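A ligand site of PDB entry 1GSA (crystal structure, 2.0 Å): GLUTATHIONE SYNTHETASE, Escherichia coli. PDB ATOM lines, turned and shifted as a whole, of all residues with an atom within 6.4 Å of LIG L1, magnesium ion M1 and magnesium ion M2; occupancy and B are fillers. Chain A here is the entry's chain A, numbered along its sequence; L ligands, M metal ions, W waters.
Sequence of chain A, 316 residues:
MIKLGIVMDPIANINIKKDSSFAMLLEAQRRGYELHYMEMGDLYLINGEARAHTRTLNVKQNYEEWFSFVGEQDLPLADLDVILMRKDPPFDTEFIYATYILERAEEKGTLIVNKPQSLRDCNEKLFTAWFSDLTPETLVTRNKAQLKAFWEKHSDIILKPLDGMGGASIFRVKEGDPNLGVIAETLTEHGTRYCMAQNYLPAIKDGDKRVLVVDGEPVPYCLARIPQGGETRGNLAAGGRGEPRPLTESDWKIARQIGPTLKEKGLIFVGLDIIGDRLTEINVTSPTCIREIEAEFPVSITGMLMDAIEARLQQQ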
ATOM      1  N   GLU A 124      -1.588  29.060  10.529  1.00  0.00           N
ATOM      2  CA  GLU A 124      -2.716  28.218  10.137  1.00  0.00           C
ATOM      3  C   GLU A 124      -3.985  28.958   9.766  1.00  0.00           C
ATOM      4  O   GLU A 124      -4.752  28.519   8.909  1.00  0.00           O
ATOM      5  CB  GLU A 124      -2.989  27.220  11.257  1.00  0.00           C
ATOM      6  CG  GLU A 124      -1.717  26.375  11.493  1.00  0.00           C
ATOM      7  CD  GLU A 124      -1.786  25.202  12.457  1.00  0.00           C
ATOM      8  OE1 GLU A 124      -2.547  25.214  13.420  1.00  0.00           O
ATOM      9  OE2 GLU A 124      -1.067  24.242  12.254  1.00  0.00           O
ATOM     10  N   LYS A 125      -4.218  30.127  10.342  1.00  0.00           N
ATOM     11  CA  LYS A 125      -5.345  30.917   9.963  1.00  0.00           C
ATOM     12  C   LYS A 125      -4.922  31.925   8.925  1.00  0.00           C
ATOM     13  O   LYS A 125      -5.574  32.000   7.885  1.00  0.00           O
ATOM     14  CB  LYS A 125      -5.949  31.681  11.124  1.00  0.00           C
ATOM     15  CG  LYS A 125      -6.520  30.896  12.279  1.00  0.00           C
ATOM     16  CD  LYS A 125      -7.456  29.769  11.856  1.00  0.00           C
ATOM     17  CE  LYS A 125      -8.085  29.103  13.094  1.00  0.00           C
ATOM     18  NZ  LYS A 125      -7.092  28.505  13.982  1.00  0.00           N
ATOM     19  N   PRO A 136     -13.897  31.598   2.740  1.00  0.00           N
ATOM     20  CA  PRO A 136     -15.009  32.525   2.893  1.00  0.00           C
ATOM     21  C   PRO A 136     -14.545  33.973   2.985  1.00  0.00           C
ATOM     22  O   PRO A 136     -13.340  34.282   2.835  1.00  0.00           O
ATOM     23  CB  PRO A 136     -15.716  32.017   4.103  1.00  0.00           C
ATOM     24  CG  PRO A 136     -14.709  31.200   4.855  1.00  0.00           C
ATOM     25  CD  PRO A 136     -13.862  30.581   3.786  1.00  0.00           C
ATOM     26  N   ILE A 158     -18.725  33.752  11.998  1.00  0.00           N
ATOM     27  CA  ILE A 158     -17.852  32.947  12.850  1.00  0.00           C
ATOM     28  C   ILE A 158     -16.694  33.895  13.228  1.00  0.00           C
ATOM     29  O   ILE A 158     -16.103  34.533  12.350  1.00  0.00           O
ATOM     30  CB  ILE A 158     -17.305  31.731  12.073  1.00  0.00           C
ATOM     31  CG1 ILE A 158     -18.412  30.740  11.811  1.00  0.00           C
ATOM     32  CG2 ILE A 158     -16.174  31.089  12.833  1.00  0.00           C
ATOM     33  CD1 ILE A 158     -19.026  30.029  13.024  1.00  0.00           C
ATOM     34  N   LYS A 160     -13.094  33.984  15.553  1.00  0.00           N
ATOM     35  CA  LYS A 160     -12.098  33.065  16.078  1.00  0.00           C
ATOM     36  C   LYS A 160     -10.781  33.740  16.396  1.00  0.00           C
ATOM     37  O   LYS A 160     -10.515  34.805  15.824  1.00  0.00           O
ATOM     38  CB  LYS A 160     -11.841  31.975  15.066  1.00  0.00           C
ATOM     39  CG  LYS A 160     -11.611  32.405  13.659  1.00  0.00           C
ATOM     40  CD  LYS A 160     -12.193  31.229  12.918  1.00  0.00           C
ATOM     41  CE  LYS A 160     -11.915  31.264  11.452  1.00  0.00           C
ATOM     42  NZ  LYS A 160     -12.230  29.937  10.954  1.00  0.00           N
ATOM     43  N   GLY A 164      -4.962  29.300  18.116  1.00  0.00           N
ATOM     44  CA  GLY A 164      -5.334  27.967  18.584  1.00  0.00           C
ATOM     45  C   GLY A 164      -5.742  27.062  17.429  1.00  0.00           C
ATOM     46  O   GLY A 164      -5.707  27.430  16.247  1.00  0.00           O
ATOM     47  N   MET A 165      -6.121  25.872  17.835  1.00  0.00           N
ATOM     48  CA  MET A 165      -6.586  24.841  16.929  1.00  0.00           C
ATOM     49  C   MET A 165      -7.634  24.064  17.724  1.00  0.00           C
ATOM     50  O   MET A 165      -7.904  24.408  18.881  1.00  0.00           O
ATOM     51  CB  MET A 165      -5.429  23.926  16.501  1.00  0.00           C
ATOM     52  CG  MET A 165      -4.930  22.803  17.415  1.00  0.00           C
ATOM     53  SD  MET A 165      -4.522  23.347  19.105  1.00  0.00           S
ATOM     54  CE  MET A 165      -4.493  21.701  19.766  1.00  0.00           C
ATOM     55  N   GLY A 166      -8.299  23.052  17.141  1.00  0.00           N
ATOM     56  CA  GLY A 166      -9.248  22.236  17.894  1.00  0.00           C
ATOM     57  C   GLY A 166     -10.559  22.905  18.343  1.00  0.00           C
ATOM     58  O   GLY A 166     -11.296  22.347  19.164  1.00  0.00           O
ATOM     59  N   GLY A 167     -10.989  24.020  17.746  1.00  0.00           N
ATOM     60  CA  GLY A 167     -12.204  24.677  18.156  1.00  0.00           C
ATOM     61  C   GLY A 167     -11.974  25.631  19.306  1.00  0.00           C
ATOM     62  O   GLY A 167     -12.936  26.023  19.986  1.00  0.00           O
ATOM     63  N   ALA A 168     -10.735  26.093  19.519  1.00  0.00           N
ATOM     64  CA  ALA A 168     -10.474  27.022  20.607  1.00  0.00           C
ATOM     65  C   ALA A 168     -11.110  28.351  20.258  1.00  0.00           C
ATOM     66  O   ALA A 168     -10.928  28.880  19.161  1.00  0.00           O
ATOM     67  CB  ALA A 168      -8.974  27.250  20.796  1.00  0.00           C
ATOM     68  N   ILE A 170     -14.241  29.445  19.243  1.00  0.00           N
ATOM     69  CA  ILE A 170     -15.032  29.756  18.053  1.00  0.00           C
ATOM     70  C   ILE A 170     -16.417  30.218  18.463  1.00  0.00           C
ATOM     71  O   ILE A 170     -17.162  29.468  19.090  1.00  0.00           O
ATOM     72  CB  ILE A 170     -15.163  28.524  17.176  1.00  0.00           C
ATOM     73  CG1 ILE A 170     -13.821  27.903  16.843  1.00  0.00           C
ATOM     74  CG2 ILE A 170     -15.897  28.958  15.933  1.00  0.00           C
ATOM     75  CD1 ILE A 170     -12.892  28.589  15.840  1.00  0.00           C
ATOM     76  N   GLN A 198     -15.339  35.428   9.830  1.00  0.00           N
ATOM     77  CA  GLN A 198     -15.562  34.855   8.519  1.00  0.00           C
ATOM     78  C   GLN A 198     -17.041  34.683   8.420  1.00  0.00           C
ATOM     79  O   GLN A 198     -17.691  34.479   9.446  1.00  0.00           O
ATOM     80  CB  GLN A 198     -15.071  33.440   8.298  1.00  0.00           C
ATOM     81  CG  GLN A 198     -13.606  33.164   8.512  1.00  0.00           C
ATOM     82  CD  GLN A 198     -13.272  31.779   8.049  1.00  0.00           C
ATOM     83  OE1 GLN A 198     -13.853  30.792   8.452  1.00  0.00           O
ATOM     84  NE2 GLN A 198     -12.327  31.672   7.132  1.00  0.00           N
ATOM     85  N   ASN A 199     -17.640  34.691   7.227  1.00  0.00           N
ATOM     86  CA  ASN A 199     -19.073  34.435   7.163  1.00  0.00           C
ATOM     87  C   ASN A 199     -19.310  32.959   7.429  1.00  0.00           C
ATOM     88  O   ASN A 199     -18.478  32.113   7.124  1.00  0.00           O
ATOM     89  CB  ASN A 199     -19.691  34.829   5.791  1.00  0.00           C
ATOM     90  CG  ASN A 199     -19.007  34.232   4.593  1.00  0.00           C
ATOM     91  OD1 ASN A 199     -17.862  34.539   4.331  1.00  0.00           O
ATOM     92  ND2 ASN A 199     -19.600  33.404   3.763  1.00  0.00           N
ATOM     93  N   TYR A 200     -20.405  32.627   8.122  1.00  0.00           N
ATOM     94  CA  TYR A 200     -20.696  31.268   8.488  1.00  0.00           C
ATOM     95  C   TYR A 200     -21.054  30.466   7.249  1.00  0.00           C
ATOM     96  O   TYR A 200     -21.751  30.947   6.358  1.00  0.00           O
ATOM     97  CB  TYR A 200     -21.826  31.314   9.509  1.00  0.00           C
ATOM     98  CG  TYR A 200     -22.453  29.986   9.884  1.00  0.00           C
ATOM     99  CD1 TYR A 200     -21.849  29.154  10.827  1.00  0.00           C
ATOM    100  CD2 TYR A 200     -23.634  29.594   9.232  1.00  0.00           C
ATOM    101  CE1 TYR A 200     -22.428  27.922  11.123  1.00  0.00           C
ATOM    102  CE2 TYR A 200     -24.226  28.366   9.532  1.00  0.00           C
ATOM    103  CZ  TYR A 200     -23.622  27.535  10.475  1.00  0.00           C
ATOM    104  OH  TYR A 200     -24.218  26.301  10.763  1.00  0.00           O
ATOM    105  N   LEU A 201     -20.575  29.230   7.196  1.00  0.00           N
ATOM    106  CA  LEU A 201     -20.798  28.329   6.091  1.00  0.00           C
ATOM    107  C   LEU A 201     -21.748  27.225   6.508  1.00  0.00           C
ATOM    108  O   LEU A 201     -21.312  26.295   7.181  1.00  0.00           O
ATOM    109  CB  LEU A 201     -19.471  27.721   5.644  1.00  0.00           C
ATOM    110  CG  LEU A 201     -18.404  28.684   5.165  1.00  0.00           C
ATOM    111  CD1 LEU A 201     -17.124  27.937   4.970  1.00  0.00           C
ATOM    112  CD2 LEU A 201     -18.827  29.325   3.875  1.00  0.00           C
ATOM    113  N   PRO A 202     -23.042  27.277   6.148  1.00  0.00           N
ATOM    114  CA  PRO A 202     -24.056  26.268   6.469  1.00  0.00           C
ATOM    115  C   PRO A 202     -23.656  24.824   6.211  1.00  0.00           C
ATOM    116  O   PRO A 202     -24.036  23.903   6.940  1.00  0.00           O
ATOM    117  CB  PRO A 202     -25.233  26.688   5.657  1.00  0.00           C
ATOM    118  CG  PRO A 202     -25.133  28.179   5.694  1.00  0.00           C
ATOM    119  CD  PRO A 202     -23.654  28.364   5.397  1.00  0.00           C
ATOM    120  N   ILE A 204     -21.215  23.248   7.090  1.00  0.00           N
ATOM    121  CA  ILE A 204     -20.578  22.573   8.200  1.00  0.00           C
ATOM    122  C   ILE A 204     -21.421  21.403   8.683  1.00  0.00           C
ATOM    123  O   ILE A 204     -20.907  20.449   9.236  1.00  0.00           O
ATOM    124  CB  ILE A 204     -20.297  23.639   9.315  1.00  0.00           C
ATOM    125  CG1 ILE A 204     -19.554  23.004  10.502  1.00  0.00           C
ATOM    126  CG2 ILE A 204     -21.609  24.237   9.805  1.00  0.00           C
ATOM    127  CD1 ILE A 204     -18.289  22.208  10.104  1.00  0.00           C
ATOM    128  N   ASP A 208     -16.705  19.221   8.541  1.00  0.00           N
ATOM    129  CA  ASP A 208     -15.510  19.999   8.301  1.00  0.00           C
ATOM    130  C   ASP A 208     -14.563  18.922   7.784  1.00  0.00           C
ATOM    131  O   ASP A 208     -14.152  18.076   8.571  1.00  0.00           O
ATOM    132  CB  ASP A 208     -14.987  20.612   9.623  1.00  0.00           C
ATOM    133  CG  ASP A 208     -13.783  21.553   9.480  1.00  0.00           C
ATOM    134  OD1 ASP A 208     -12.930  21.377   8.612  1.00  0.00           O
ATOM    135  OD2 ASP A 208     -13.650  22.506  10.236  1.00  0.00           O
ATOM    136  N   ARG A 210     -11.130  17.183   6.865  1.00  0.00           N
ATOM    137  CA  ARG A 210      -9.696  17.285   6.955  1.00  0.00           C
ATOM    138  C   ARG A 210      -9.182  16.584   5.712  1.00  0.00           C
ATOM    139  O   ARG A 210      -9.414  15.378   5.546  1.00  0.00           O
ATOM    140  CB  ARG A 210      -9.211  16.584   8.214  1.00  0.00           C
ATOM    141  CG  ARG A 210      -7.698  16.265   8.253  1.00  0.00           C
ATOM    142  CD  ARG A 210      -6.746  17.439   7.919  1.00  0.00           C
ATOM    143  NE  ARG A 210      -7.017  18.602   8.728  1.00  0.00           N
ATOM    144  CZ  ARG A 210      -6.795  18.649  10.043  1.00  0.00           C
ATOM    145  NH1 ARG A 210      -6.291  17.653  10.748  1.00  0.00           N
ATOM    146  NH2 ARG A 210      -7.166  19.700  10.725  1.00  0.00           N
ATOM    147  N   ARG A 225     -15.640  15.973   9.642  1.00  0.00           N
ATOM    148  CA  ARG A 225     -15.881  16.056  11.076  1.00  0.00           C
ATOM    149  C   ARG A 225     -17.216  16.759  11.279  1.00  0.00           C
ATOM    150  O   ARG A 225     -17.422  17.927  10.906  1.00  0.00           O
ATOM    151  CB  ARG A 225     -14.734  16.843  11.755  1.00  0.00           C
ATOM    152  CG  ARG A 225     -13.382  16.149  11.733  1.00  0.00           C
ATOM    153  CD  ARG A 225     -12.429  16.873  10.793  1.00  0.00           C
ATOM    154  NE  ARG A 225     -11.425  17.579  11.560  1.00  0.00           N
ATOM    155  CZ  ARG A 225     -10.963  18.774  11.261  1.00  0.00           C
ATOM    156  NH1 ARG A 225     -11.359  19.504  10.217  1.00  0.00           N
ATOM    157  NH2 ARG A 225     -10.048  19.239  12.077  1.00  0.00           N
ATOM    158  N   PRO A 227     -20.074  18.271  13.731  1.00  0.00           N
ATOM    159  CA  PRO A 227     -20.301  18.806  15.075  1.00  0.00           C
ATOM    160  C   PRO A 227     -21.351  17.948  15.768  1.00  0.00           C
ATOM    161  O   PRO A 227     -22.204  17.361  15.082  1.00  0.00           O
ATOM    162  CB  PRO A 227     -20.761  20.227  14.881  1.00  0.00           C
ATOM    163  CG  PRO A 227     -20.215  20.580  13.518  1.00  0.00           C
ATOM    164  CD  PRO A 227     -20.381  19.281  12.731  1.00  0.00           C
ATOM    165  N   THR A 232     -21.159  23.959  17.905  1.00  0.00           N
ATOM    166  CA  THR A 232     -20.758  24.714  16.741  1.00  0.00           C
ATOM    167  C   THR A 232     -19.410  24.247  16.221  1.00  0.00           C
ATOM    168  O   THR A 232     -19.001  24.629  15.109  1.00  0.00           O
ATOM    169  CB  THR A 232     -20.723  26.183  17.175  1.00  0.00           C
ATOM    170  OG1 THR A 232     -22.005  26.369  17.774  1.00  0.00           O
ATOM    171  CG2 THR A 232     -20.489  27.187  16.071  1.00  0.00           C
ATOM    172  N   ARG A 233     -18.637  23.448  16.976  1.00  0.00           N
ATOM    173  CA  ARG A 233     -17.354  23.006  16.472  1.00  0.00           C
ATOM    174  C   ARG A 233     -17.372  21.576  15.919  1.00  0.00           C
ATOM    175  O   ARG A 233     -17.827  20.663  16.617  1.00  0.00           O
ATOM    176  CB  ARG A 233     -16.293  23.124  17.567  1.00  0.00           C
ATOM    177  CG  ARG A 233     -16.001  24.574  17.750  1.00  0.00           C
ATOM    178  CD  ARG A 233     -16.659  25.081  19.005  1.00  0.00           C
ATOM    179  NE  ARG A 233     -15.677  24.951  20.052  1.00  0.00           N
ATOM    180  CZ  ARG A 233     -15.929  24.926  21.360  1.00  0.00           C
ATOM    181  NH1 ARG A 233     -17.148  24.982  21.915  1.00  0.00           N
ATOM    182  NH2 ARG A 233     -14.855  24.911  22.156  1.00  0.00           N
ATOM    183  N   GLY A 234     -16.911  21.421  14.668  1.00  0.00           N
ATOM    184  CA  GLY A 234     -16.769  20.136  14.000  1.00  0.00           C
ATOM    185  C   GLY A 234     -15.564  19.350  14.499  1.00  0.00           C
ATOM    186  O   GLY A 234     -15.552  18.134  14.452  1.00  0.00           O
ATOM    187  N   ASN A 235     -14.507  20.030  14.955  1.00  0.00           N
ATOM    188  CA  ASN A 235     -13.289  19.439  15.512  1.00  0.00           C
ATOM    189  C   ASN A 235     -13.450  18.186  16.328  1.00  0.00           C
ATOM    190  O   ASN A 235     -14.243  18.189  17.267  1.00  0.00           O
ATOM    191  CB  ASN A 235     -12.560  20.397  16.432  1.00  0.00           C
ATOM    192  CG  ASN A 235     -12.247  21.685  15.735  1.00  0.00           C
ATOM    193  OD1 ASN A 235     -13.062  22.603  15.716  1.00  0.00           O
ATOM    194  ND2 ASN A 235     -11.064  21.815  15.152  1.00  0.00           N
ATOM    195  N   ASP A 273      -8.392  22.145   5.954  1.00  0.00           N
ATOM    196  CA  ASP A 273      -9.727  22.049   6.501  1.00  0.00           C
ATOM    197  C   ASP A 273     -10.677  22.549   5.411  1.00  0.00           C
ATOM    198  O   ASP A 273     -10.489  23.687   4.975  1.00  0.00           O
ATOM    199  CB  ASP A 273      -9.846  22.925   7.712  1.00  0.00           C
ATOM    200  CG  ASP A 273      -9.404  22.319   9.025  1.00  0.00           C
ATOM    201  OD1 ASP A 273      -8.560  21.434   9.046  1.00  0.00           O
ATOM    202  OD2 ASP A 273      -9.919  22.760  10.048  1.00  0.00           O
ATOM    203  N   ILE A 275     -14.781  23.259   4.312  1.00  0.00           N
ATOM    204  CA  ILE A 275     -16.190  23.146   4.684  1.00  0.00           C
ATOM    205  C   ILE A 275     -16.887  23.466   3.357  1.00  0.00           C
ATOM    206  O   ILE A 275     -16.739  24.564   2.795  1.00  0.00           O
ATOM    207  CB  ILE A 275     -16.587  24.181   5.750  1.00  0.00           C
ATOM    208  CG1 ILE A 275     -16.008  23.842   7.100  1.00  0.00           C
ATOM    209  CG2 ILE A 275     -18.087  24.226   5.854  1.00  0.00           C
ATOM    210  CD1 ILE A 275     -16.317  24.894   8.185  1.00  0.00           C
ATOM    211  N   THR A 280     -11.083  26.754   5.043  1.00  0.00           N
ATOM    212  CA  THR A 280     -11.120  27.601   6.222  1.00  0.00           C
ATOM    213  C   THR A 280      -9.780  27.742   6.935  1.00  0.00           C
ATOM    214  O   THR A 280      -9.504  28.839   7.389  1.00  0.00           O
ATOM    215  CB  THR A 280     -12.176  27.067   7.137  1.00  0.00           C
ATOM    216  OG1 THR A 280     -11.936  25.673   7.280  1.00  0.00           O
ATOM    217  CG2 THR A 280     -13.556  27.366   6.605  1.00  0.00           C
ATOM    218  N   GLU A 281      -8.892  26.747   7.025  1.00  0.00           N
ATOM    219  CA  GLU A 281      -7.574  26.955   7.576  1.00  0.00           C
ATOM    220  C   GLU A 281      -6.593  25.948   6.994  1.00  0.00           C
ATOM    221  O   GLU A 281      -7.034  24.997   6.339  1.00  0.00           O
ATOM    222  CB  GLU A 281      -7.635  26.830   9.089  1.00  0.00           C
ATOM    223  CG  GLU A 281      -7.499  25.454   9.659  1.00  0.00           C
ATOM    224  CD  GLU A 281      -7.586  25.428  11.163  1.00  0.00           C
ATOM    225  OE1 GLU A 281      -7.110  26.329  11.847  1.00  0.00           O
ATOM    226  OE2 GLU A 281      -8.161  24.472  11.668  1.00  0.00           O
ATOM    227  N   ILE A 282      -5.279  26.175   7.157  1.00  0.00           N
ATOM    228  CA  ILE A 282      -4.202  25.261   6.687  1.00  0.00           C
ATOM    229  C   ILE A 282      -3.280  24.772   7.837  1.00  0.00           C
ATOM    230  O   ILE A 282      -2.357  25.457   8.275  1.00  0.00           O
ATOM    231  CB  ILE A 282      -3.371  26.005   5.573  1.00  0.00           C
ATOM    232  CG1 ILE A 282      -4.275  26.426   4.418  1.00  0.00           C
ATOM    233  CG2 ILE A 282      -2.311  25.085   5.017  1.00  0.00           C
ATOM    234  CD1 ILE A 282      -3.621  27.108   3.194  1.00  0.00           C
ATOM    235  N   ASN A 283      -3.452  23.566   8.376  1.00  0.00           N
ATOM    236  CA  ASN A 283      -2.660  23.105   9.492  1.00  0.00           C
ATOM    237  C   ASN A 283      -1.352  22.539   9.029  1.00  0.00           C
ATOM    238  O   ASN A 283      -1.256  21.531   8.338  1.00  0.00           O
ATOM    239  CB  ASN A 283      -3.407  22.056  10.327  1.00  0.00           C
ATOM    240  CG  ASN A 283      -4.663  22.737  10.849  1.00  0.00           C
ATOM    241  OD1 ASN A 283      -4.609  23.779  11.494  1.00  0.00           O
ATOM    242  ND2 ASN A 283      -5.874  22.326  10.540  1.00  0.00           N
HETATM  243  P1  LIG L   1      -9.462  25.474  14.471  1.00  0.00           P
HETATM  244  O1  LIG L   1      -7.973  25.587  14.360  1.00  0.00           O
HETATM  245  O2  LIG L   1      -9.801  25.688  15.903  1.00  0.00           O
HETATM  246  O3  LIG L   1      -9.856  24.107  14.033  1.00  0.00           O
HETATM  247  P2  LIG L   1     -11.190  26.362  12.344  1.00  0.00           P
HETATM  248  O4  LIG L   1     -10.847  25.130  11.585  1.00  0.00           O
HETATM  249  O5  LIG L   1     -11.095  27.481  11.380  1.00  0.00           O
HETATM  250  O6  LIG L   1     -10.229  26.584  13.595  1.00  0.00           O
HETATM  251  O7  LIG L   1     -12.680  26.279  12.967  1.00  0.00           O
HETATM  252  C1  LIG L   1     -12.990  25.305  13.966  1.00  0.00           C
HETATM  253  C2  LIG L   1     -14.462  24.968  13.933  1.00  0.00           C
HETATM  254  O8  LIG L   1     -15.282  26.159  13.971  1.00  0.00           O
HETATM  255  C3  LIG L   1     -14.773  24.316  12.585  1.00  0.00           C
HETATM  256  O9  LIG L   1     -14.634  22.905  12.635  1.00  0.00           O
HETATM  257  C4  LIG L   1     -16.226  24.657  12.381  1.00  0.00           C
HETATM  258  O10 LIG L   1     -17.045  23.816  13.193  1.00  0.00           O
HETATM  259  C5  LIG L   1     -16.268  26.080  12.923  1.00  0.00           C
HETATM  260  N1  LIG L   1     -15.985  27.012  11.819  1.00  0.00           N
HETATM  261  C6  LIG L   1     -14.859  27.735  11.547  1.00  0.00           C
HETATM  262  N2  LIG L   1     -15.017  28.582  10.464  1.00  0.00           N
HETATM  263  C7  LIG L   1     -16.328  28.347  10.074  1.00  0.00           C
HETATM  264  C8  LIG L   1     -17.118  28.911   9.056  1.00  0.00           C
HETATM  265  N3  LIG L   1     -16.670  29.884   8.265  1.00  0.00           N
HETATM  266  N4  LIG L   1     -18.376  28.463   8.932  1.00  0.00           N
HETATM  267  C9  LIG L   1     -18.828  27.526   9.775  1.00  0.00           C
HETATM  268  N5  LIG L   1     -18.198  26.929  10.764  1.00  0.00           N
HETATM  269  C10 LIG L   1     -16.913  27.397  10.873  1.00  0.00           C
HETATM  270  S1  LG2 L   2      -7.812  21.684  13.647  1.00  0.00           S
HETATM  271  O1  LG2 L   2      -6.720  20.990  13.053  1.00  0.00           O
HETATM  272  O2  LG2 L   2      -7.374  22.977  14.098  1.00  0.00           O
HETATM  273  O3  LG2 L   2      -8.285  20.988  14.838  1.00  0.00           O
HETATM  274  O4  LG2 L   2      -8.821  21.725  12.603  1.00  0.00           O
HETATM  275  N1  LG3 L   3      -0.442  15.931  17.824  1.00  0.00           N
HETATM  276  C1  LG3 L   3      -1.746  15.345  17.607  1.00  0.00           C
HETATM  277  C2  LG3 L   3      -1.816  14.052  16.823  1.00  0.00           C
HETATM  278  O1  LG3 L   3      -0.883  13.751  16.068  1.00  0.00           O
HETATM  279  O2  LG3 L   3      -2.834  13.363  16.944  1.00  0.00           O
HETATM  280  C3  LG3 L   3      -2.629  16.345  16.911  1.00  0.00           C
HETATM  281  C4  LG3 L   3      -3.064  17.476  17.799  1.00  0.00           C
HETATM  282  C5  LG3 L   3      -4.094  18.353  17.111  1.00  0.00           C
HETATM  283  O3  LG3 L   3      -5.191  18.586  17.657  1.00  0.00           O
HETATM  284  N2  LG3 L   3      -3.787  18.821  15.893  1.00  0.00           N
HETATM  285  C6  LG3 L   3      -4.729  19.643  15.169  1.00  0.00           C
HETATM  286  C7  LG3 L   3      -5.647  18.705  14.398  1.00  0.00           C
HETATM  287  O4  LG3 L   3      -5.280  18.152  13.360  1.00  0.00           O
HETATM  288  C8  LG3 L   3      -4.012  20.535  14.183  1.00  0.00           C
HETATM  289  S1  LG3 L   3      -2.541  21.220  14.943  1.00  0.00           S
HETATM  290  N3  LG3 L   3      -6.875  18.560  14.888  1.00  0.00           N
HETATM  291  C9  LG3 L   3      -7.887  17.764  14.204  1.00  0.00           C
HETATM  292  C10 LG3 L   3      -9.230  17.775  14.923  1.00  0.00           C
HETATM  293  O5  LG3 L   3      -9.363  18.240  16.069  1.00  0.00           O
HETATM  294  O6  LG3 L   3     -10.177  17.281  14.307  1.00  0.00           O
HETATM  295 MG    MG M   1      -9.822  23.459  11.937  1.00  0.00          MG
HETATM  296 MG    MG M   2      -6.377  24.038  12.872  1.00  0.00          MG
HETATM  297  O   HOH W   1      -5.038  25.696  13.990  1.00  0.00           O
HETATM  298  O   HOH W   2     -11.607  22.420  12.343  1.00  0.00           O
HETATM  299  O   HOH W   3      -9.043  28.070  17.426  1.00  0.00           O
HETATM  300  O   HOH W   4     -12.894  25.221   9.954  1.00  0.00           O
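The side-chain amino group of Lys 125 is in salt-bridge range of the side-chain carboxylate of Glu 281 (3.0 Å). ND2 of Asn 283 lies within hydrogen-bond range of OD1 of Asp 273 (3.2 Å). The side-chain carboxylate (OD1) of Asp 273 lies within salt-bridge range of the guanidinium group (NH1) of Arg 225 (3.6 Å). The side-chain carboxylate (OD1) of Asp 273 lies within salt-bridge range of the guanidinium group (NH2) of Arg 210 (2.8 Å). OD1 of Asn 283 sits close to OE1 of Glu 124, at 3.2 Å. The side-chain carboxylate of Asp 208 lies within salt-bridge range of the guanidinium group of Arg 225 (2.9 Å). The backbone carbonyl oxygen of Ile 158 is in hydrogen-bond range of the backbone NH of Gln 198, 2.8 Å away. The side-chain amino group (NZ) of Lys 125 lies within hydrogen-bond range of the backbone carbonyl oxygen (O) of Gly 164.
Magnesium ion M1 is bound by the side-chain carboxylate of Glu 281 (2.0 Å), an oxygen (O4) of LIG L1 (2.0 Å), the side-chain carboxylate of Asp 273 (2.0 Å), water W2 (2.1 Å), an oxygen (O4) of LG2 L2 (2.1 Å) and an oxygen (O3) of LIG L1 (2.2 Å). Magnesium ion M1 has six donor atoms within binding distance.
Water W2 lies within hydrogen-bond range of the side-chain amide nitrogen (ND2) of Asn 235 (2.9 Å), the side-chain carboxylate (OD2) of Asp 208 (2.9 Å) and an oxygen (O9) of LIG L1 (3.1 Å). Water W4 lies within hydrogen-bond range of OD2 of Asp 208 (2.8 Å), OG1 of Thr 280 (2.9 Å) and O7 of LIG L1 (3.2 Å). Water W3 bridges the backbone carbonyl oxygen of Ala 168 (2.7 Å) and an oxygen (O2) of LIG L1 (2.9 Å).
Magnesium ion M2 is bound by an oxygen (O2) of LG2 L2 (1.9 Å), the side-chain carboxylate of Glu 281 (2.2 Å), the side-chain amide oxygen of Asn 283 (2.3 Å) and water W1 (2.4 Å). Magnesium ion M2 has four donor atoms within binding distance. Slightly farther from magnesium ion M2 lies the side-chain carboxylate (OE1) of Glu 281 (2.6 Å). Slightly farther from magnesium ion M2 lies an oxygen (O1) of LIG L1 (2.7 Å).
O1 of LIG L1 lies close to O of Gly 164 (3.5 Å). Merely in contact with LIG L1: Met 165, Arg 233, Ile 170, Ile 158, Tyr 200, Ile 204, Ile 275 and Ala 168. Within 4 Å of LIG L1: Lys 125, Ile 158, Lys 160, Gly 164, Met 165, Gly 166, Gly 167, Ala 168, Ile 170, Gln 198, Asn 199, Tyr 200, Leu 201, Ile 204, Asp 208, Thr 232, Arg 233, Gly 234, Asn 235, Asp 273, Ile 275 and Glu 281. The nearest printed residue that does not touch LIG L1 is Pro 136 (4.1 Å).
Asn 235 touches magnesium ion M1. Of the 31 residues printed, 3 come within 4 Å of magnesium ion M1. The nearest printed residue that does not touch magnesium ion M1 is Arg 225 (4.2 Å).
An oxygen (O9) of LIG L1 sits at hydrogen-bond distance from the side-chain carboxylate of Asp 208, at 2.6 Å. The side-chain amino group (NZ) of Lys 160 lies within salt-bridge range of an oxygen (O5) of LIG L1, 2.7 Å away. The backbone NH of Gly 167 is in hydrogen-bond range of an oxygen (O2) of LIG L1, at 2.8 Å. An oxygen (O10) of LIG L1 is in hydrogen-bond range of the backbone NH (N) of Gly 234 (2.8 Å). OD1 of Asn 235 lies close to O9 of LIG L1, at 3.5 Å. O of Thr 232 sits at hydrogen-bond distance from O10 of LIG L1 (2.9 Å). The backbone NH (N) of Leu 201 is in hydrogen-bond range of a nitrogen (N4) of LIG L1 (2.9 Å). N3 of LIG L1 lies within hydrogen-bond range of OE1 of Gln 198, 3.0 Å away. NZ of Lys 125 lies within salt-bridge range of O1 of LIG L1 (3.1 Å). The backbone carbonyl oxygen of Asn 199 is in hydrogen-bond range of a nitrogen (N3) of LIG L1. The backbone NH (N) of Gly 166 is in hydrogen-bond range of an oxygen (O2) of LIG L1, at 3.3 Å. O6 of LG3 L3 lies within salt-bridge range of NH2 of Arg 225 (3.0 Å). An oxygen (O4) of LG3 L3 sits at hydrogen-bond distance from the guanidinium group (NH1) of Arg 210 (2.8 Å).
Merely in contact with magnesium ion M2: Met 165. Of the 31 residues printed, 3 come within 4 Å of magnesium ion M2.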
